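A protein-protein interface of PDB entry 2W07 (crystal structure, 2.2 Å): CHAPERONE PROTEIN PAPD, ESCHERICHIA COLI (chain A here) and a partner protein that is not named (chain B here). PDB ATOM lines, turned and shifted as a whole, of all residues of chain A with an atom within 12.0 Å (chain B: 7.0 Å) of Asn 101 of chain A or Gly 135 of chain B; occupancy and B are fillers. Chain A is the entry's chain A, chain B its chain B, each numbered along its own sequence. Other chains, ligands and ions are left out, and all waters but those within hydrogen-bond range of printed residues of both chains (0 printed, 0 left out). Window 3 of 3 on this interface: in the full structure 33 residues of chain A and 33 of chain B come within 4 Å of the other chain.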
ATOM      1  N   PRO A  95      14.213 -24.654 -10.292  1.00  0.00           N
ATOM      2  CA  PRO A  95      13.389 -23.476 -10.574  1.00  0.00           C
ATOM      3  C   PRO A  95      13.368 -22.548  -9.359  1.00  0.00           C
ATOM      4  O   PRO A  95      13.404 -23.007  -8.217  1.00  0.00           O
ATOM      5  CB  PRO A  95      12.024 -24.085 -10.876  1.00  0.00           C
ATOM      6  CG  PRO A  95      11.993 -25.272  -9.963  1.00  0.00           C
ATOM      7  CD  PRO A  95      13.378 -25.860 -10.147  1.00  0.00           C
ATOM      8  N   ARG A  96      13.317 -21.245  -9.613  1.00  0.00           N
ATOM      9  CA  ARG A  96      13.305 -20.252  -8.545  1.00  0.00           C
ATOM     10  C   ARG A  96      12.126 -20.421  -7.598  1.00  0.00           C
ATOM     11  O   ARG A  96      10.975 -20.299  -8.003  1.00  0.00           O
ATOM     12  CB  ARG A  96      13.277 -18.841  -9.138  1.00  0.00           C
ATOM     13  CG  ARG A  96      13.448 -17.740  -8.107  1.00  0.00           C
ATOM     14  CD  ARG A  96      13.471 -16.369  -8.755  1.00  0.00           C
ATOM     15  NE  ARG A  96      13.926 -15.340  -7.823  1.00  0.00           N
ATOM     16  CZ  ARG A  96      13.987 -14.042  -8.108  1.00  0.00           C
ATOM     17  NH1 ARG A  96      13.618 -13.605  -9.305  1.00  0.00           N
ATOM     18  NH2 ARG A  96      14.426 -13.181  -7.199  1.00  0.00           N
ATOM     19  N   SER A  97      12.423 -20.698  -6.334  1.00  0.00           N
ATOM     20  CA  SER A  97      11.389 -20.871  -5.321  1.00  0.00           C
ATOM     21  C   SER A  97      10.565 -19.592  -5.214  1.00  0.00           C
ATOM     22  O   SER A  97      11.115 -18.492  -5.255  1.00  0.00           O
ATOM     23  CB  SER A  97      12.038 -21.185  -3.966  1.00  0.00           C
ATOM     24  OG  SER A  97      11.078 -21.275  -2.927  1.00  0.00           O
ATOM     25  N   GLU A  98       9.247 -19.728  -5.095  1.00  0.00           N
ATOM     26  CA  GLU A  98       8.397 -18.551  -4.973  1.00  0.00           C
ATOM     27  C   GLU A  98       8.603 -17.925  -3.600  1.00  0.00           C
ATOM     28  O   GLU A  98       8.589 -16.703  -3.456  1.00  0.00           O
ATOM     29  CB  GLU A  98       6.920 -18.909  -5.156  1.00  0.00           C
ATOM     30  CG  GLU A  98       5.985 -17.783  -4.730  1.00  0.00           C
ATOM     31  CD  GLU A  98       4.540 -18.041  -5.092  1.00  0.00           C
ATOM     32  OE1 GLU A  98       4.213 -17.991  -6.293  1.00  0.00           O
ATOM     33  OE2 GLU A  98       3.730 -18.292  -4.174  1.00  0.00           O
ATOM     34  N   LYS A  99       8.796 -18.777  -2.597  1.00  0.00           N
ATOM     35  CA  LYS A  99       9.015 -18.325  -1.227  1.00  0.00           C
ATOM     36  C   LYS A  99      10.409 -17.722  -1.075  1.00  0.00           C
ATOM     37  O   LYS A  99      11.407 -18.348  -1.437  1.00  0.00           O
ATOM     38  CB  LYS A  99       8.848 -19.492  -0.258  1.00  0.00           C
ATOM     39  N   ALA A 100      10.468 -16.505  -0.545  1.00  0.00           N
ATOM     40  CA  ALA A 100      11.739 -15.819  -0.329  1.00  0.00           C
ATOM     41  C   ALA A 100      12.316 -16.250   1.019  1.00  0.00           C
ATOM     42  O   ALA A 100      11.674 -16.990   1.768  1.00  0.00           O
ATOM     43  CB  ALA A 100      11.533 -14.308  -0.359  1.00  0.00           C
ATOM     44  N   ASN A 101      13.521 -15.779   1.329  1.00  0.00           N
ATOM     45  CA  ASN A 101      14.192 -16.140   2.577  1.00  0.00           C
ATOM     46  C   ASN A 101      14.405 -17.649   2.595  1.00  0.00           C
ATOM     47  O   ASN A 101      13.977 -18.348   3.519  1.00  0.00           O
ATOM     48  CB  ASN A 101      13.358 -15.716   3.789  1.00  0.00           C
ATOM     49  CG  ASN A 101      13.132 -14.220   3.841  1.00  0.00           C
ATOM     50  OD1 ASN A 101      14.025 -13.436   3.524  1.00  0.00           O
ATOM     51  ND2 ASN A 101      11.934 -13.818   4.254  1.00  0.00           N
ATOM     52  N   VAL A 102      15.075 -18.142   1.560  1.00  0.00           N
ATOM     53  CA  VAL A 102      15.334 -19.565   1.429  1.00  0.00           C
ATOM     54  C   VAL A 102      16.736 -19.872   0.932  1.00  0.00           C
ATOM     55  O   VAL A 102      17.403 -19.034   0.316  1.00  0.00           O
ATOM     56  CB  VAL A 102      14.357 -20.215   0.432  1.00  0.00           C
ATOM     57  CG1 VAL A 102      12.937 -20.150   0.965  1.00  0.00           C
ATOM     58  CG2 VAL A 102      14.455 -19.503  -0.915  1.00  0.00           C
ATOM     59  N   LEU A 103      17.169 -21.092   1.213  1.00  0.00           N
ATOM     60  CA  LEU A 103      18.463 -21.573   0.765  1.00  0.00           C
ATOM     61  C   LEU A 103      18.096 -22.675  -0.220  1.00  0.00           C
ATOM     62  O   LEU A 103      17.485 -23.673   0.161  1.00  0.00           O
ATOM     63  CB  LEU A 103      19.264 -22.178   1.926  1.00  0.00           C
ATOM     64  CG  LEU A 103      20.773 -22.392   1.741  1.00  0.00           C
ATOM     65  CD1 LEU A 103      21.236 -23.484   2.686  1.00  0.00           C
ATOM     66  CD2 LEU A 103      21.109 -22.781   0.307  1.00  0.00           C
ATOM     67  N   GLN A 104      18.438 -22.491  -1.486  1.00  0.00           N
ATOM     68  CA  GLN A 104      18.133 -23.509  -2.476  1.00  0.00           C
ATOM     69  C   GLN A 104      19.353 -24.368  -2.737  1.00  0.00           C
ATOM     70  O   GLN A 104      20.454 -23.856  -2.952  1.00  0.00           O
ATOM     71  CB  GLN A 104      17.648 -22.874  -3.781  1.00  0.00           C
ATOM     72  CG  GLN A 104      16.249 -22.295  -3.668  1.00  0.00           C
ATOM     73  CD  GLN A 104      15.652 -21.952  -5.014  1.00  0.00           C
ATOM     74  OE1 GLN A 104      15.567 -22.805  -5.898  1.00  0.00           O
ATOM     75  NE2 GLN A 104      15.225 -20.702  -5.175  1.00  0.00           N
ATOM     76  N   ILE A 105      19.153 -25.678  -2.695  1.00  0.00           N
ATOM     77  CA  ILE A 105      20.238 -26.613  -2.940  1.00  0.00           C
ATOM     78  C   ILE A 105      20.206 -27.075  -4.392  1.00  0.00           C
ATOM     79  O   ILE A 105      19.173 -27.521  -4.895  1.00  0.00           O
ATOM     80  CB  ILE A 105      20.132 -27.855  -2.029  1.00  0.00           C
ATOM     81  CG1 ILE A 105      20.272 -27.448  -0.556  1.00  0.00           C
ATOM     82  CG2 ILE A 105      21.190 -28.871  -2.415  1.00  0.00           C
ATOM     83  CD1 ILE A 105      21.551 -26.702  -0.226  1.00  0.00           C
ATOM     84  N   VAL B  25      15.775 -24.949   1.874  1.00  0.00           N
ATOM     85  CA  VAL B  25      15.790 -24.669   3.302  1.00  0.00           C
ATOM     86  C   VAL B  25      15.079 -23.330   3.478  1.00  0.00           C
ATOM     87  O   VAL B  25      15.619 -22.284   3.115  1.00  0.00           O
ATOM     88  CB  VAL B  25      17.228 -24.545   3.833  1.00  0.00           C
ATOM     89  CG1 VAL B  25      17.212 -24.441   5.347  1.00  0.00           C
ATOM     90  CG2 VAL B  25      18.057 -25.735   3.378  1.00  0.00           C
ATOM     91  N   ASP B  26      13.865 -23.369   4.020  1.00  0.00           N
ATOM     92  CA  ASP B  26      13.074 -22.160   4.229  1.00  0.00           C
ATOM     93  C   ASP B  26      13.259 -21.612   5.637  1.00  0.00           C
ATOM     94  O   ASP B  26      13.177 -22.349   6.618  1.00  0.00           O
ATOM     95  CB  ASP B  26      11.596 -22.451   3.972  1.00  0.00           C
ATOM     96  N   PHE B  27      13.511 -20.312   5.730  1.00  0.00           N
ATOM     97  CA  PHE B  27      13.709 -19.669   7.020  1.00  0.00           C
ATOM     98  C   PHE B  27      12.459 -18.904   7.433  1.00  0.00           C
ATOM     99  O   PHE B  27      12.464 -18.161   8.412  1.00  0.00           O
ATOM    100  CB  PHE B  27      14.911 -18.722   6.958  1.00  0.00           C
ATOM    101  CG  PHE B  27      16.189 -19.400   6.566  1.00  0.00           C
ATOM    102  CD1 PHE B  27      16.433 -19.738   5.238  1.00  0.00           C
ATOM    103  CD2 PHE B  27      17.131 -19.746   7.527  1.00  0.00           C
ATOM    104  CE1 PHE B  27      17.595 -20.414   4.877  1.00  0.00           C
ATOM    105  CE2 PHE B  27      18.294 -20.421   7.174  1.00  0.00           C
ATOM    106  CZ  PHE B  27      18.526 -20.756   5.846  1.00  0.00           C
ATOM    107  N   GLY B  28      11.385 -19.098   6.678  1.00  0.00           N
ATOM    108  CA  GLY B  28      10.142 -18.417   6.982  1.00  0.00           C
ATOM    109  C   GLY B  28      10.278 -16.913   6.865  1.00  0.00           C
ATOM    110  O   GLY B  28      11.165 -16.413   6.172  1.00  0.00           O
ATOM    111  N   ASN B  29       9.400 -16.185   7.546  1.00  0.00           N
ATOM    112  CA  ASN B  29       9.437 -14.734   7.497  1.00  0.00           C
ATOM    113  C   ASN B  29      10.174 -14.188   8.714  1.00  0.00           C
ATOM    114  O   ASN B  29       9.613 -14.092   9.808  1.00  0.00           O
ATOM    115  CB  ASN B  29       8.015 -14.170   7.446  1.00  0.00           C
ATOM    116  CG  ASN B  29       7.947 -12.835   6.727  1.00  0.00           C
ATOM    117  OD1 ASN B  29       8.604 -11.870   7.119  1.00  0.00           O
ATOM    118  ND2 ASN B  29       7.152 -12.776   5.662  1.00  0.00           N
ATOM    119  N   ILE B  30      11.441 -13.837   8.513  1.00  0.00           N
ATOM    120  CA  ILE B  30      12.268 -13.306   9.587  1.00  0.00           C
ATOM    121  C   ILE B  30      12.995 -12.050   9.128  1.00  0.00           C
ATOM    122  O   ILE B  30      13.316 -11.908   7.950  1.00  0.00           O
ATOM    123  CB  ILE B  30      13.318 -14.338  10.041  1.00  0.00           C
ATOM    124  CG1 ILE B  30      14.311 -14.602   8.905  1.00  0.00           C
ATOM    125  CG2 ILE B  30      12.626 -15.631  10.465  1.00  0.00           C
ATOM    126  CD1 ILE B  30      15.473 -15.484   9.295  1.00  0.00           C
ATOM    127  N   ASN B  31      13.247 -11.140  10.063  1.00  0.00           N
ATOM    128  CA  ASN B  31      13.950  -9.904   9.745  1.00  0.00           C
ATOM    129  C   ASN B  31      15.440 -10.211   9.744  1.00  0.00           C
ATOM    130  O   ASN B  31      15.964 -10.749  10.718  1.00  0.00           O
ATOM    131  CB  ASN B  31      13.651  -8.829  10.793  1.00  0.00           C
ATOM    132  CG  ASN B  31      14.194  -7.464  10.399  1.00  0.00           C
ATOM    133  OD1 ASN B  31      15.367  -7.325  10.052  1.00  0.00           O
ATOM    134  ND2 ASN B  31      13.339  -6.448  10.457  1.00  0.00           N
ATOM    135  N   PRO B  32      16.142  -9.880   8.647  1.00  0.00           N
ATOM    136  CA  PRO B  32      17.583 -10.130   8.540  1.00  0.00           C
ATOM    137  C   PRO B  32      18.401  -9.608   9.728  1.00  0.00           C
ATOM    138  O   PRO B  32      19.625  -9.738   9.752  1.00  0.00           O
ATOM    139  CB  PRO B  32      17.947  -9.445   7.226  1.00  0.00           C
ATOM    140  CG  PRO B  32      16.716  -9.673   6.401  1.00  0.00           C
ATOM    141  CD  PRO B  32      15.612  -9.341   7.381  1.00  0.00           C
ATOM    142  N   ASN B  77      21.774 -12.485  -1.308  1.00  0.00           N
ATOM    143  CA  ASN B  77      21.530 -11.338  -2.175  1.00  0.00           C
ATOM    144  C   ASN B  77      21.386 -10.088  -1.317  1.00  0.00           C
ATOM    145  O   ASN B  77      20.718  -9.124  -1.694  1.00  0.00           O
ATOM    146  CB  ASN B  77      20.274 -11.561  -3.029  1.00  0.00           C
ATOM    147  CG  ASN B  77      19.015 -11.723  -2.199  1.00  0.00           C
ATOM    148  OD1 ASN B  77      18.965 -12.529  -1.270  1.00  0.00           O
ATOM    149  ND2 ASN B  77      17.981 -10.961  -2.541  1.00  0.00           N
ATOM    150  N   ILE B  78      22.020 -10.127  -0.149  1.00  0.00           N
ATOM    151  CA  ILE B  78      22.013  -9.016   0.796  1.00  0.00           C
ATOM    152  C   ILE B  78      23.435  -8.838   1.311  1.00  0.00           C
ATOM    153  O   ILE B  78      24.020  -9.765   1.869  1.00  0.00           O
ATOM    154  CB  ILE B  78      21.087  -9.288   1.998  1.00  0.00           C
ATOM    155  CG1 ILE B  78      19.637  -9.389   1.529  1.00  0.00           C
ATOM    156  CG2 ILE B  78      21.228  -8.174   3.025  1.00  0.00           C
ATOM    157  CD1 ILE B  78      18.626  -9.506   2.661  1.00  0.00           C
ATOM    158  N   PHE B  81      25.110 -10.089   4.779  1.00  0.00           N
ATOM    159  CA  PHE B  81      24.196 -11.098   5.292  1.00  0.00           C
ATOM    160  C   PHE B  81      24.428 -12.436   4.591  1.00  0.00           C
ATOM    161  O   PHE B  81      24.445 -12.510   3.362  1.00  0.00           O
ATOM    162  CB  PHE B  81      22.753 -10.658   5.079  1.00  0.00           C
ATOM    163  CG  PHE B  81      21.747 -11.639   5.598  1.00  0.00           C
ATOM    164  CD1 PHE B  81      21.460 -11.703   6.954  1.00  0.00           C
ATOM    165  CD2 PHE B  81      21.116 -12.526   4.736  1.00  0.00           C
ATOM    166  CE1 PHE B  81      20.560 -12.640   7.443  1.00  0.00           C
ATOM    167  CE2 PHE B  81      20.217 -13.465   5.218  1.00  0.00           C
ATOM    168  CZ  PHE B  81      19.940 -13.522   6.573  1.00  0.00           C
ATOM    169  N   LEU B 132      20.831  -3.052   6.599  1.00  0.00           N
ATOM    170  CA  LEU B 132      20.963  -4.066   5.561  1.00  0.00           C
ATOM    171  C   LEU B 132      19.983  -3.744   4.441  1.00  0.00           C
ATOM    172  O   LEU B 132      18.784  -3.593   4.680  1.00  0.00           O
ATOM    173  CB  LEU B 132      20.655  -5.459   6.118  1.00  0.00           C
ATOM    174  CG  LEU B 132      21.602  -6.053   7.163  1.00  0.00           C
ATOM    175  CD1 LEU B 132      21.088  -7.424   7.585  1.00  0.00           C
ATOM    176  CD2 LEU B 132      23.007  -6.157   6.594  1.00  0.00           C
ATOM    177  N   ASN B 133      20.500  -3.636   3.222  1.00  0.00           N
ATOM    178  CA  ASN B 133      19.674  -3.334   2.063  1.00  0.00           C
ATOM    179  C   ASN B 133      18.906  -4.564   1.587  1.00  0.00           C
ATOM    180  O   ASN B 133      19.337  -5.262   0.672  1.00  0.00           O
ATOM    181  CB  ASN B 133      20.541  -2.784   0.925  1.00  0.00           C
ATOM    182  CG  ASN B 133      21.722  -3.685   0.594  1.00  0.00           C
ATOM    183  OD1 ASN B 133      21.552  -4.838   0.205  1.00  0.00           O
ATOM    184  ND2 ASN B 133      22.929  -3.155   0.747  1.00  0.00           N
ATOM    185  N   GLY B 134      17.765  -4.828   2.218  1.00  0.00           N
ATOM    186  CA  GLY B 134      16.965  -5.971   1.825  1.00  0.00           C
ATOM    187  C   GLY B 134      16.204  -6.616   2.965  1.00  0.00           C
ATOM    188  O   GLY B 134      16.766  -6.880   4.027  1.00  0.00           O
ATOM    189  N   GLY B 135      14.917  -6.864   2.736  1.00  0.00           N
ATOM    190  CA  GLY B 135      14.084  -7.491   3.746  1.00  0.00           C
ATOM    191  C   GLY B 135      13.909  -8.957   3.407  1.00  0.00           C
ATOM    192  O   GLY B 135      13.582  -9.777   4.267  1.00  0.00           O
ATOM    193  N   ASP B 136      14.128  -9.276   2.134  1.00  0.00           N
ATOM    194  CA  ASP B 136      14.024 -10.640   1.630  1.00  0.00           C
ATOM    195  C   ASP B 136      15.404 -11.075   1.171  1.00  0.00           C
ATOM    196  O   ASP B 136      16.205 -10.246   0.733  1.00  0.00           O
ATOM    197  CB  ASP B 136      13.059 -10.713   0.441  1.00  0.00           C
ATOM    198  CG  ASP B 136      11.607 -10.659   0.861  1.00  0.00           C
ATOM    199  OD1 ASP B 136      11.179 -11.540   1.636  1.00  0.00           O
ATOM    200  OD2 ASP B 136      10.889  -9.740   0.410  1.00  0.00           O
ATOM    201  N   PHE B 137      15.683 -12.371   1.267  1.00  0.00           N
ATOM    202  CA  PHE B 137      16.977 -12.891   0.848  1.00  0.00           C
ATOM    203  C   PHE B 137      16.840 -14.294   0.285  1.00  0.00           C
ATOM    204  O   PHE B 137      15.917 -15.027   0.627  1.00  0.00           O
ATOM    205  CB  PHE B 137      17.957 -12.916   2.029  1.00  0.00           C
ATOM    206  CG  PHE B 137      17.754 -14.079   2.966  1.00  0.00           C
ATOM    207  CD1 PHE B 137      18.239 -15.345   2.643  1.00  0.00           C
ATOM    208  CD2 PHE B 137      17.055 -13.916   4.155  1.00  0.00           C
ATOM    209  CE1 PHE B 137      18.027 -16.431   3.491  1.00  0.00           C
ATOM    210  CE2 PHE B 137      16.839 -14.998   5.010  1.00  0.00           C
ATOM    211  CZ  PHE B 137      17.326 -16.257   4.676  1.00  0.00           C
ATOM    212  N   ARG B 138      17.776 -14.654  -0.580  1.00  0.00           N
ATOM    213  CA  ARG B 138      17.807 -15.971  -1.188  1.00  0.00           C
ATOM    214  C   ARG B 138      19.226 -16.255  -1.655  1.00  0.00           C
ATOM    215  O   ARG B 138      19.951 -15.348  -2.064  1.00  0.00           O
ATOM    216  CB  ARG B 138      16.818 -16.058  -2.358  1.00  0.00           C
ATOM    217  CG  ARG B 138      16.709 -14.804  -3.208  1.00  0.00           C
ATOM    218  CD  ARG B 138      15.540 -14.910  -4.185  1.00  0.00           C
ATOM    219  NE  ARG B 138      14.307 -15.323  -3.515  1.00  0.00           N
ATOM    220  CZ  ARG B 138      13.120 -15.418  -4.109  1.00  0.00           C
ATOM    221  NH1 ARG B 138      12.991 -15.126  -5.396  1.00  0.00           N
ATOM    222  NH2 ARG B 138      12.058 -15.804  -3.415  1.00  0.00           N
ATOM    223  N   THR B 139      19.625 -17.516  -1.570  1.00  0.00           N
ATOM    224  CA  THR B 139      20.960 -17.914  -1.980  1.00  0.00           C
ATOM    225  C   THR B 139      20.921 -19.351  -2.468  1.00  0.00           C
ATOM    226  O   THR B 139      19.936 -20.063  -2.247  1.00  0.00           O
ATOM    227  CB  THR B 139      21.950 -17.776  -0.807  1.00  0.00           C
ATOM    228  OG1 THR B 139      23.250 -18.213  -1.220  1.00  0.00           O
ATOM    229  CG2 THR B 139      21.484 -18.593   0.379  1.00  0.00           C
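CB of Ala 100 of chain A touches OD1 of Asp 136 of chain B (3.4 Å). C of Ala 100 of chain A touches O of Phe 137 of chain B, 3.8 Å away. Asn 101 of chain A touches Asp 26 of chain B (O to C, 3.96 Å). Asn 101 of chain A touches Gly 135 of chain B (OD1 to O, 3.8 Å). Asn 101 of chain A touches Asp 136 of chain B. CA of Asp 26 of chain B touches CG1 of Val 102 of chain A, at 3.8 Å. Phe 27 of chain B touches Val 102 of chain A. Arg 138 of chain B touches Val 102 of chain A. N of Leu 103 of chain A touches CE1 of Phe 27 of chain B, 3.8 Å away. CA of Leu 103 of chain A touches O of Thr 139 of chain B, at 3.7 Å.
Of the printed residues of chain B, Arg 96 of chain A touches Arg 138. Of the printed residues of chain B, Ala 100 of chain A touches Asp 136, Phe 137 and Arg 138. Printed residues of chain B within 4 Å of Val 102 of chain A: Val 25 (3.2 Å), Asp 26 (3.8 Å), Phe 27 (3.97 Å), Phe 137 (3.4 Å), Arg 138 (3.4 Å) and Thr 139 (3.3 Å). Of the printed residues of chain B, Leu 103 of chain A touches Val 25, Phe 27 and Thr 139. Printed residues of chain A within 4 Å of Asp 26 of chain B: Asn 101 and Val 102. Gly 28 of chain B touches just one residue of chain A: Asn 101 (3.3 Å). No residue of chain A comes within 4 Å of Asn 31 of chain B. Phe 81 of chain B touches none of the printed residues of chain A. No residue of chain A comes within 4 Å of Gly 134 of chain B. Of chain A, only Asn 101 comes within 4 Å of Gly 135 of chain B. Asp 136 of chain B touches just these residues of chain A: Ala 100 (3.4 Å) and Asn 101 (3.4 Å). Phe 137 of chain B touches just these residues of chain A: Ala 100 (3.8 Å), Asn 101 (2.6 Å) and Val 102 (3.4 Å). Of the printed residues of chain A, Thr 139 of chain B touches Val 102 (3.3 Å), Leu 103 (3.7 Å) and Gln 104 (3.0 Å). The nearest residue of chain B that does not touch Asn 101 of chain A is Asn 29 of chain B (4.2 Å).
Printed residues of chain B that touch a printed residue of chain A: Val 25, Asp 26, Phe 27, Gly 28, Gly 135, Asp 136, Phe 137, Arg 138 and Thr 139. Hydrophobic or aromatic side chains of chain B within 4 Å of the printed part of chain A: Val 25, Phe 27 and Phe 137. Printed residues of chain A that touch a printed residue of chain B: Arg 96, Ser 97, Glu 98, Lys 99, Ala 100, Asn 101, Val 102, Leu 103 and Gln 104. Hydrophobic or aromatic side chains of chain A within 4 Å of the printed part of chain B: Ala 100, Val 102 and Leu 103.
The backbone carbonyl oxygen (O) of Phe 137 of chain B sits at hydrogen-bond distance from the backbone NH (N) of Val 102 of chain A, 3.4 Å away. O of Val 25 of chain B is in hydrogen-bond range of N of Leu 103 of chain A (2.7 Å). O of Val 102 of chain A is in hydrogen-bond range of N of Thr 139 of chain B (3.3 Å). O of Gly 28 of chain B lies close to ND2 of Asn 101 of chain A (3.3 Å). N of Ala 100 of chain A lies close to NH2 of Arg 138 of chain B, at 3.4 Å. The backbone carbonyl oxygen (O) of Ser 97 of chain A sits at hydrogen-bond distance from the guanidinium group (NH2) of Arg 138 of chain B, 3.4 Å away. The backbone NH (N) of Asn 101 of chain A is in hydrogen-bond range of the backbone carbonyl oxygen (O) of Phe 137 of chain B (2.6 Å). N of Gln 104 of chain A lies within hydrogen-bond range of O of Thr 139 of chain B. NE of Arg 96 of chain A lies close to NH1 of Arg 138 of chain B. NH2 of Arg 138 of chain B sits at hydrogen-bond distance from O of Lys 99 of chain A (3.3 Å). N of Phe 27 of chain B sits at hydrogen-bond distance from O of Asn 101 of chain A, at 3.0 Å.
The backbone carbonyl oxygen (O) of Pro 95 of chain A lies close to the side-chain amide oxygen (OE1) of Gln 104 of chain A, 3.2 Å away. OD1 of Asn 77 of chain B lies within hydrogen-bond range of N of Arg 138 of chain B. The backbone NH of Ser 97 of chain A lies close to the side-chain amide nitrogen of Gln 104 of chain A (3.0 Å). The side-chain hydroxyl (OG) of Ser 97 of chain A lies within hydrogen-bond range of the backbone carbonyl oxygen (O) of Lys 99 of chain A (3.3 Å).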
